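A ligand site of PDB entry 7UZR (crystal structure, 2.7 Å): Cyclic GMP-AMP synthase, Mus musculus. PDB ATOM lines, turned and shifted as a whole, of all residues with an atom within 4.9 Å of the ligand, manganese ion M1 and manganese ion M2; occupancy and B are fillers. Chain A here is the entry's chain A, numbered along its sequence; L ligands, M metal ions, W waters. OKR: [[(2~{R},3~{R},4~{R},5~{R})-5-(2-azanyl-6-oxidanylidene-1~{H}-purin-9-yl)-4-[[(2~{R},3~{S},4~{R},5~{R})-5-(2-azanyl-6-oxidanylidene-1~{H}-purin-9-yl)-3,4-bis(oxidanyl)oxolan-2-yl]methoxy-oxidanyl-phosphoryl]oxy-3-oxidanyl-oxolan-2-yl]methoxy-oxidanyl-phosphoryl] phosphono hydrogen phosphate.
Gly 55 touches the ligand (CA to O12, 3.2 Å). Lys 62 touches the ligand. Lys 145 touches the ligand (CE to O19, 3.1 Å). CE of Lys 266 touches N3 of the ligand, at 3.7 Å. Phe 275 touches the ligand (O to N3, 3.9 Å). CB of Tyr 278 touches C17 of the ligand, 3.6 Å away. Hydrophobic or aromatic side chains that line the ligand: Tyr 278. 13 residues have an atom within 4 Å of the ligand: Gly 55, Ser 56, Lys 62, Glu 68, Asp 70, Lys 145, Arg 221, Lys 259, Lys 266, Phe 275, Cys 276, Ser 277 and Tyr 278.
Water W1 lies within hydrogen-bond range of the side-chain hydroxyl (OG) of Ser 56 and the backbone carbonyl oxygen (O) of Glu 68. Water W3 bridges OE1 of Glu 59 (2.7 Å) and O11 of the ligand (2.8 Å). Water W2 lies within hydrogen-bond range of an oxygen (O16) of the ligand (2.8 Å), the side-chain amino group of Lys 62 (3.1 Å) and the side-chain carboxylate of Glu 263 (3.2 Å).
Manganese ion M2 is bound by the side-chain carboxylate (OE1) of Glu 68. The side-chain carboxylate (OD2) of Asp 70 binds manganese ion M2, at 2.1 Å. Manganese ion M2 is bound by O14 of the ligand. Manganese ion M2 is bound by water W1 (2.3 Å). O9 of the ligand binds manganese ion M2 (2.3 Å). O12 of the ligand is bound to manganese ion M2 (2.4 Å). Manganese ion M2 has six donor atoms within binding distance.
The side-chain carboxylate (OD2) of Asp 164 binds manganese ion M1 (1.9 Å). OE2 of Glu 68 binds manganese ion M1 (2.0 Å). Manganese ion M1 is bound by OD1 of Asp 70. Manganese ion M1 is bound by an oxygen (O9) of the ligand, at 2.4 Å. Manganese ion M1 has four donor atoms within binding distance.
The side-chain sulfur of Cys 276 lies close to the backbone NH of Tyr 278 (3.6 Å). The backbone carbonyl oxygen (O) of Phe 275 is in hydrogen-bond range of the side-chain amino group (NZ) of Lys 266 (3.0 Å). The backbone carbonyl oxygen (O) of Ser 56 lies within hydrogen-bond range of the backbone NH (N) of Lys 62 (3.3 Å). The side-chain hydroxyl (OH) of Tyr 278 sits at hydrogen-bond distance from a ring nitrogen (NE2) of His 324, at 3.4 Å.
Merely in contact with manganese ion M2: Ser 56 (3.6 Å). Three residues have an atom within 4 Å of manganese ion M2: Ser 56, Glu 68 and Asp 70. The nearest printed residue that does not touch manganese ion M2 is Gly 55 (4.9 Å).
Of the 20 residues printed, 3 come within 4 Å of manganese ion M1.
SG of Cys 276 lies within hydrogen-bond range of O17 of the ligand. The side-chain hydroxyl (OG) of Ser 56 is in hydrogen-bond range of an oxygen (O16) of the ligand, 2.7 Å away. NH1 of Arg 221 is in hydrogen-bond range of O18 of the ligand (2.7 Å). The side-chain amino group of Lys 259 lies within salt-bridge range of an oxygen (O16) of the ligand (3.2 Å). O15 of the ligand sits at hydrogen-bond distance from OG of Ser 277, at 2.8 Å. O12 of the ligand lies close to N of Ser 56, 2.8 Å away. An oxygen (O21) of the ligand lies within hydrogen-bond range of the backbone NH (N) of Ser 277 (3.0 Å).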
ATOM      1  N   GLY A  55      23.063  33.436   9.933  1.00  0.00           N
ATOM      2  CA  GLY A  55      24.102  32.596   9.401  1.00  0.00           C
ATOM      3  C   GLY A  55      25.268  33.386   8.850  1.00  0.00           C
ATOM      4  O   GLY A  55      25.294  34.625   8.903  1.00  0.00           O
ATOM      5  N   SER A  56      26.208  32.641   8.260  1.00  0.00           N
ATOM      6  CA  SER A  56      27.512  33.131   7.861  1.00  0.00           C
ATOM      7  C   SER A  56      27.444  34.267   6.881  1.00  0.00           C
ATOM      8  O   SER A  56      28.254  35.186   6.972  1.00  0.00           O
ATOM      9  CB  SER A  56      28.345  31.981   7.268  1.00  0.00           C
ATOM     10  OG  SER A  56      27.666  31.335   6.163  1.00  0.00           O
ATOM     11  N   GLU A  59      26.476  37.381   8.547  1.00  0.00           N
ATOM     12  CA  GLU A  59      27.531  37.666   9.538  1.00  0.00           C
ATOM     13  C   GLU A  59      28.877  38.068   8.884  1.00  0.00           C
ATOM     14  O   GLU A  59      29.843  38.423   9.567  1.00  0.00           O
ATOM     15  CB  GLU A  59      27.771  36.451  10.422  1.00  0.00           C
ATOM     16  CG  GLU A  59      26.641  36.080  11.367  1.00  0.00           C
ATOM     17  CD  GLU A  59      26.749  34.671  11.993  1.00  0.00           C
ATOM     18  OE1 GLU A  59      27.633  33.857  11.566  1.00  0.00           O
ATOM     19  OE2 GLU A  59      25.922  34.385  12.909  1.00  0.00           O
ATOM     20  N   LYS A  62      30.956  33.984   5.483  1.00  0.00           N
ATOM     21  CA  LYS A  62      30.784  33.000   4.428  1.00  0.00           C
ATOM     22  C   LYS A  62      32.023  32.986   3.570  1.00  0.00           C
ATOM     23  O   LYS A  62      32.477  34.034   3.120  1.00  0.00           O
ATOM     24  CB  LYS A  62      29.579  33.358   3.562  1.00  0.00           C
ATOM     25  CG  LYS A  62      29.225  32.355   2.494  1.00  0.00           C
ATOM     26  CD  LYS A  62      28.602  31.128   3.108  1.00  0.00           C
ATOM     27  CE  LYS A  62      28.385  30.042   2.064  1.00  0.00           C
ATOM     28  NZ  LYS A  62      29.661  29.547   1.490  1.00  0.00           N
ATOM     29  N   GLU A  68      25.279  29.326   0.098  1.00  0.00           N
ATOM     30  CA  GLU A  68      24.410  28.859   1.158  1.00  0.00           C
ATOM     31  C   GLU A  68      23.982  30.095   1.971  1.00  0.00           C
ATOM     32  O   GLU A  68      24.795  30.905   2.338  1.00  0.00           O
ATOM     33  CB  GLU A  68      25.054  27.744   2.024  1.00  0.00           C
ATOM     34  CG  GLU A  68      24.062  26.851   2.813  1.00  0.00           C
ATOM     35  CD  GLU A  68      23.829  27.259   4.261  1.00  0.00           C
ATOM     36  OE1 GLU A  68      24.352  28.324   4.665  1.00  0.00           O
ATOM     37  OE2 GLU A  68      23.123  26.526   5.012  1.00  0.00           O
ATOM     38  N   ASP A  70      21.031  31.322   5.062  1.00  0.00           N
ATOM     39  CA  ASP A  70      20.138  30.841   6.089  1.00  0.00           C
ATOM     40  C   ASP A  70      19.117  31.965   6.406  1.00  0.00           C
ATOM     41  O   ASP A  70      19.496  33.106   6.524  1.00  0.00           O
ATOM     42  CB  ASP A  70      20.965  30.394   7.294  1.00  0.00           C
ATOM     43  CG  ASP A  70      22.083  29.384   6.913  1.00  0.00           C
ATOM     44  OD1 ASP A  70      21.795  28.214   6.600  1.00  0.00           O
ATOM     45  OD2 ASP A  70      23.257  29.765   6.936  1.00  0.00           O
ATOM     46  N   LYS A 145      15.746  15.947   5.244  1.00  0.00           N
ATOM     47  CA  LYS A 145      16.777  15.268   5.992  1.00  0.00           C
ATOM     48  C   LYS A 145      16.258  15.166   7.411  1.00  0.00           C
ATOM     49  O   LYS A 145      15.844  16.171   7.992  1.00  0.00           O
ATOM     50  CB  LYS A 145      18.051  16.094   6.006  1.00  0.00           C
ATOM     51  CG  LYS A 145      18.645  16.218   4.625  1.00  0.00           C
ATOM     52  CD  LYS A 145      20.094  16.631   4.708  1.00  0.00           C
ATOM     53  CE  LYS A 145      20.634  17.082   3.361  1.00  0.00           C
ATOM     54  NZ  LYS A 145      20.066  16.332   2.208  1.00  0.00           N
ATOM     55  N   GLY A 147      16.435  15.067  11.482  1.00  0.00           N
ATOM     56  CA  GLY A 147      17.210  15.901  12.380  1.00  0.00           C
ATOM     57  C   GLY A 147      17.533  17.259  11.797  1.00  0.00           C
ATOM     58  O   GLY A 147      18.532  17.856  12.188  1.00  0.00           O
ATOM     59  N   ASP A 164      18.392  27.512   3.408  1.00  0.00           N
ATOM     60  CA  ASP A 164      17.652  26.900   4.478  1.00  0.00           C
ATOM     61  C   ASP A 164      16.589  27.887   4.939  1.00  0.00           C
ATOM     62  O   ASP A 164      16.922  28.947   5.469  1.00  0.00           O
ATOM     63  CB  ASP A 164      18.596  26.553   5.619  1.00  0.00           C
ATOM     64  CG  ASP A 164      19.634  25.535   5.227  1.00  0.00           C
ATOM     65  OD1 ASP A 164      19.311  24.677   4.363  1.00  0.00           O
ATOM     66  OD2 ASP A 164      20.763  25.600   5.797  1.00  0.00           O
ATOM     67  N   ARG A 221      14.007  22.823  19.812  1.00  0.00           N
ATOM     68  CA  ARG A 221      15.406  23.150  20.229  1.00  0.00           C
ATOM     69  C   ARG A 221      15.575  24.682  20.201  1.00  0.00           C
ATOM     70  O   ARG A 221      15.052  25.306  19.263  1.00  0.00           O
ATOM     71  CB  ARG A 221      16.436  22.485  19.304  1.00  0.00           C
ATOM     72  CG  ARG A 221      17.887  22.620  19.753  1.00  0.00           C
ATOM     73  CD  ARG A 221      18.902  22.159  18.718  1.00  0.00           C
ATOM     74  NE  ARG A 221      18.849  22.957  17.495  1.00  0.00           N
ATOM     75  CZ  ARG A 221      19.394  24.172  17.308  1.00  0.00           C
ATOM     76  NH1 ARG A 221      20.065  24.749  18.297  1.00  0.00           N
ATOM     77  NH2 ARG A 221      19.264  24.797  16.149  1.00  0.00           N
ATOM     78  N   SER A 225      20.500  32.386  16.976  1.00  0.00           N
ATOM     79  CA  SER A 225      21.081  32.883  15.728  1.00  0.00           C
ATOM     80  C   SER A 225      21.107  34.394  15.649  1.00  0.00           C
ATOM     81  O   SER A 225      22.022  34.959  15.063  1.00  0.00           O
ATOM     82  CB  SER A 225      20.294  32.377  14.563  1.00  0.00           C
ATOM     83  OG  SER A 225      20.749  31.110  14.209  1.00  0.00           O
ATOM     84  N   LYS A 259      36.877  27.576   9.630  1.00  0.00           N
ATOM     85  CA  LYS A 259      35.721  27.080   8.868  1.00  0.00           C
ATOM     86  C   LYS A 259      36.190  26.304   7.638  1.00  0.00           C
ATOM     87  O   LYS A 259      35.613  25.245   7.300  1.00  0.00           O
ATOM     88  CB  LYS A 259      34.835  28.225   8.386  1.00  0.00           C
ATOM     89  CG  LYS A 259      33.930  28.805   9.438  1.00  0.00           C
ATOM     90  CD  LYS A 259      33.322  30.119   8.957  1.00  0.00           C
ATOM     91  CE  LYS A 259      32.158  29.921   7.956  1.00  0.00           C
ATOM     92  NZ  LYS A 259      30.870  29.437   8.573  1.00  0.00           N
ATOM     93  N   GLU A 263      35.702  22.462   6.443  1.00  0.00           N
ATOM     94  CA  GLU A 263      35.060  22.194   5.136  1.00  0.00           C
ATOM     95  C   GLU A 263      35.897  21.317   4.193  1.00  0.00           C
ATOM     96  O   GLU A 263      35.394  20.348   3.650  1.00  0.00           O
ATOM     97  CB  GLU A 263      34.723  23.497   4.382  1.00  0.00           C
ATOM     98  CG  GLU A 263      33.441  24.175   4.847  1.00  0.00           C
ATOM     99  CD  GLU A 263      33.093  25.419   4.041  1.00  0.00           C
ATOM    100  OE1 GLU A 263      33.519  25.468   2.873  1.00  0.00           O
ATOM    101  OE2 GLU A 263      32.397  26.322   4.598  1.00  0.00           O
ATOM    102  N   LYS A 266      36.088  17.871   5.622  1.00  0.00           N
ATOM    103  CA  LYS A 266      34.787  17.255   5.503  1.00  0.00           C
ATOM    104  C   LYS A 266      34.484  16.784   4.073  1.00  0.00           C
ATOM    105  O   LYS A 266      33.861  15.727   3.908  1.00  0.00           O
ATOM    106  CB  LYS A 266      33.696  18.215   5.950  1.00  0.00           C
ATOM    107  CG  LYS A 266      33.629  18.541   7.429  1.00  0.00           C
ATOM    108  CD  LYS A 266      32.384  18.017   8.134  1.00  0.00           C
ATOM    109  CE  LYS A 266      31.087  18.635   7.629  1.00  0.00           C
ATOM    110  NZ  LYS A 266      30.086  17.520   7.707  1.00  0.00           N
ATOM    111  N   PHE A 275      30.711  16.209  12.403  1.00  0.00           N
ATOM    112  CA  PHE A 275      31.165  17.569  12.661  1.00  0.00           C
ATOM    113  C   PHE A 275      30.565  18.624  11.732  1.00  0.00           C
ATOM    114  O   PHE A 275      30.242  18.331  10.605  1.00  0.00           O
ATOM    115  CB  PHE A 275      32.662  17.639  12.590  1.00  0.00           C
ATOM    116  CG  PHE A 275      33.350  16.735  13.548  1.00  0.00           C
ATOM    117  CD1 PHE A 275      33.523  17.118  14.862  1.00  0.00           C
ATOM    118  CD2 PHE A 275      33.873  15.533  13.116  1.00  0.00           C
ATOM    119  CE1 PHE A 275      34.165  16.285  15.751  1.00  0.00           C
ATOM    120  CE2 PHE A 275      34.539  14.713  13.991  1.00  0.00           C
ATOM    121  CZ  PHE A 275      34.679  15.083  15.316  1.00  0.00           C
ATOM    122  N   CYS A 276      30.412  19.848  12.250  1.00  0.00           N
ATOM    123  CA  CYS A 276      29.789  20.955  11.531  1.00  0.00           C
ATOM    124  C   CYS A 276      30.473  22.259  11.910  1.00  0.00           C
ATOM    125  O   CYS A 276      31.228  22.320  12.855  1.00  0.00           O
ATOM    126  CB  CYS A 276      28.290  21.008  11.823  1.00  0.00           C
ATOM    127  SG  CYS A 276      27.839  21.404  13.533  1.00  0.00           S
ATOM    128  N   SER A 277      30.149  23.334  11.175  1.00  0.00           N
ATOM    129  CA  SER A 277      30.762  24.629  11.407  1.00  0.00           C
ATOM    130  C   SER A 277      30.312  25.214  12.731  1.00  0.00           C
ATOM    131  O   SER A 277      30.995  26.099  13.285  1.00  0.00           O
ATOM    132  CB  SER A 277      30.459  25.588  10.267  1.00  0.00           C
ATOM    133  OG  SER A 277      29.080  25.580  10.019  1.00  0.00           O
ATOM    134  N   TYR A 278      29.169  24.771  13.241  1.00  0.00           N
ATOM    135  CA  TYR A 278      28.647  25.316  14.514  1.00  0.00           C
ATOM    136  C   TYR A 278      29.648  24.972  15.630  1.00  0.00           C
ATOM    137  O   TYR A 278      29.777  25.754  16.587  1.00  0.00           O
ATOM    138  CB  TYR A 278      27.250  24.813  14.867  1.00  0.00           C
ATOM    139  CG  TYR A 278      26.656  25.661  15.966  1.00  0.00           C
ATOM    140  CD1 TYR A 278      26.350  26.983  15.702  1.00  0.00           C
ATOM    141  CD2 TYR A 278      26.505  25.194  17.261  1.00  0.00           C
ATOM    142  CE1 TYR A 278      25.832  27.806  16.679  1.00  0.00           C
ATOM    143  CE2 TYR A 278      25.991  26.009  18.267  1.00  0.00           C
ATOM    144  CZ  TYR A 278      25.662  27.326  17.966  1.00  0.00           C
ATOM    145  OH  TYR A 278      25.153  28.171  18.900  1.00  0.00           O
ATOM    146  N   LYS A 281      32.340  27.590  15.420  1.00  0.00           N
ATOM    147  CA  LYS A 281      31.783  28.896  15.826  1.00  0.00           C
ATOM    148  C   LYS A 281      31.662  28.981  17.352  1.00  0.00           C
ATOM    149  O   LYS A 281      32.059  29.974  17.964  1.00  0.00           O
ATOM    150  CB  LYS A 281      30.409  29.081  15.224  1.00  0.00           C
ATOM    151  CG  LYS A 281      29.829  30.473  15.350  1.00  0.00           C
ATOM    152  CD  LYS A 281      28.355  30.478  14.972  1.00  0.00           C
ATOM    153  CE  LYS A 281      27.984  31.719  14.175  1.00  0.00           C
ATOM    154  NZ  LYS A 281      26.536  32.082  14.291  1.00  0.00           N
ATOM    155  N   HIS A 324      27.879  24.254  24.678  1.00  0.00           N
ATOM    156  CA  HIS A 324      27.097  25.278  23.981  1.00  0.00           C
ATOM    157  C   HIS A 324      27.353  26.602  24.701  1.00  0.00           C
ATOM    158  O   HIS A 324      27.367  26.663  25.923  1.00  0.00           O
ATOM    159  CB  HIS A 324      25.614  24.930  24.018  1.00  0.00           C
ATOM    160  CG  HIS A 324      24.808  25.625  22.974  1.00  0.00           C
ATOM    161  ND1 HIS A 324      24.502  26.963  23.057  1.00  0.00           N
ATOM    162  CD2 HIS A 324      24.253  25.178  21.824  1.00  0.00           C
ATOM    163  CE1 HIS A 324      23.785  27.303  22.000  1.00  0.00           C
ATOM    164  NE2 HIS A 324      23.622  26.242  21.240  1.00  0.00           N
HETATM  165  N1  OKR L   1      26.038  24.929   5.828  1.00  0.00           N
HETATM  166  C1  OKR L   1      26.539  23.841   6.444  1.00  0.00           C
HETATM  167  N2  OKR L   1      25.827  22.716   6.458  1.00  0.00           N
HETATM  168  C2  OKR L   1      26.465  21.720   7.111  1.00  0.00           C
HETATM  169  C3  OKR L   1      27.695  21.743   7.735  1.00  0.00           C
HETATM  170  N3  OKR L   1      27.991  20.506   8.297  1.00  0.00           N
HETATM  171  C4  OKR L   1      26.946  19.767   8.018  1.00  0.00           C
HETATM  172  N4  OKR L   1      25.980  20.455   7.302  1.00  0.00           N
HETATM  173  C5  OKR L   1      24.688  19.973   6.804  1.00  0.00           C
HETATM  174  O1  OKR L   1      23.731  20.097   7.833  1.00  0.00           O
HETATM  175  C6  OKR L   1      22.655  19.158   7.596  1.00  0.00           C
HETATM  176  C7  OKR L   1      22.318  18.439   8.884  1.00  0.00           C
HETATM  177  O2  OKR L   1      22.333  19.371  10.002  1.00  0.00           O
HETATM  178  P1  OKR L   1      23.532  19.387  11.072  1.00  0.00           P
HETATM  179  O3  OKR L   1      22.913  19.460  12.436  1.00  0.00           O
HETATM  180  O4  OKR L   1      24.515  18.264  10.838  1.00  0.00           O
HETATM  181  O5  OKR L   1      24.283  20.749  10.688  1.00  0.00           O
HETATM  182  C8  OKR L   1      23.935  21.907  11.454  1.00  0.00           C
HETATM  183  C9  OKR L   1      24.023  23.127  10.565  1.00  0.00           C
HETATM  184  O6  OKR L   1      23.568  22.874   9.241  1.00  0.00           O
HETATM  185  C10 OKR L   1      25.528  23.426  10.616  1.00  0.00           C
HETATM  186  C11 OKR L   1      25.933  24.825  10.224  1.00  0.00           C
HETATM  187  O7  OKR L   1      25.090  25.283   9.148  1.00  0.00           O
HETATM  188  P2  OKR L   1      24.627  26.814   9.064  1.00  0.00           P
HETATM  189  O8  OKR L   1      23.620  27.038  10.145  1.00  0.00           O
HETATM  190  O9  OKR L   1      24.279  27.171   7.658  1.00  0.00           O
HETATM  191  O10 OKR L   1      26.002  27.566   9.424  1.00  0.00           O
HETATM  192  P3  OKR L   1      26.579  29.059   9.349  1.00  0.00           P
HETATM  193  O11 OKR L   1      26.886  29.494  10.754  1.00  0.00           O
HETATM  194  O12 OKR L   1      25.706  29.923   8.490  1.00  0.00           O
HETATM  195  O13 OKR L   1      27.925  28.780   8.549  1.00  0.00           O
HETATM  196  P4  OKR L   1      28.130  27.979   7.164  1.00  0.00           P
HETATM  197  O14 OKR L   1      26.743  27.656   6.690  1.00  0.00           O
HETATM  198  O15 OKR L   1      28.936  26.754   7.534  1.00  0.00           O
HETATM  199  O16 OKR L   1      28.862  28.893   6.197  1.00  0.00           O
HETATM  200  O17 OKR L   1      25.871  23.172  12.001  1.00  0.00           O
HETATM  201  C12 OKR L   1      25.005  22.184  12.521  1.00  0.00           C
HETATM  202  N5  OKR L   1      24.461  22.631  13.795  1.00  0.00           N
HETATM  203  C13 OKR L   1      24.398  21.874  14.939  1.00  0.00           C
HETATM  204  N6  OKR L   1      23.858  22.497  15.961  1.00  0.00           N
HETATM  205  C14 OKR L   1      23.533  23.749  15.442  1.00  0.00           C
HETATM  206  C15 OKR L   1      22.913  24.857  16.089  1.00  0.00           C
HETATM  207  O18 OKR L   1      22.538  24.942  17.266  1.00  0.00           O
HETATM  208  N7  OKR L   1      22.760  25.932  15.216  1.00  0.00           N
HETATM  209  C16 OKR L   1      23.165  25.944  13.902  1.00  0.00           C
HETATM  210  N8  OKR L   1      22.944  27.076  13.215  1.00  0.00           N
HETATM  211  N9  OKR L   1      23.748  24.913  13.288  1.00  0.00           N
HETATM  212  C17 OKR L   1      23.890  23.850  14.117  1.00  0.00           C
HETATM  213  C18 OKR L   1      23.119  18.257   6.430  1.00  0.00           C
HETATM  214  O19 OKR L   1      22.545  18.642   5.183  1.00  0.00           O
HETATM  215  C19 OKR L   1      24.640  18.502   6.399  1.00  0.00           C
HETATM  216  O20 OKR L   1      25.187  18.279   5.122  1.00  0.00           O
HETATM  217  C20 OKR L   1      28.451  22.948   7.710  1.00  0.00           C
HETATM  218  O21 OKR L   1      29.567  23.156   8.203  1.00  0.00           O
HETATM  219  N10 OKR L   1      27.778  23.967   7.027  1.00  0.00           N
HETATM  220 MN    MN M   1      22.280  26.160   6.792  1.00  0.00          MN
HETATM  221 MN    MN M   2      25.059  28.931   6.370  1.00  0.00          MN
HETATM  222  O   HOH W   1      25.143  30.963   5.350  1.00  0.00           O
HETATM  223  O   HOH W   2      30.969  29.226   4.331  1.00  0.00           O
HETATM  224  O   HOH W   3      28.820  31.549  10.770  1.00  0.00           O
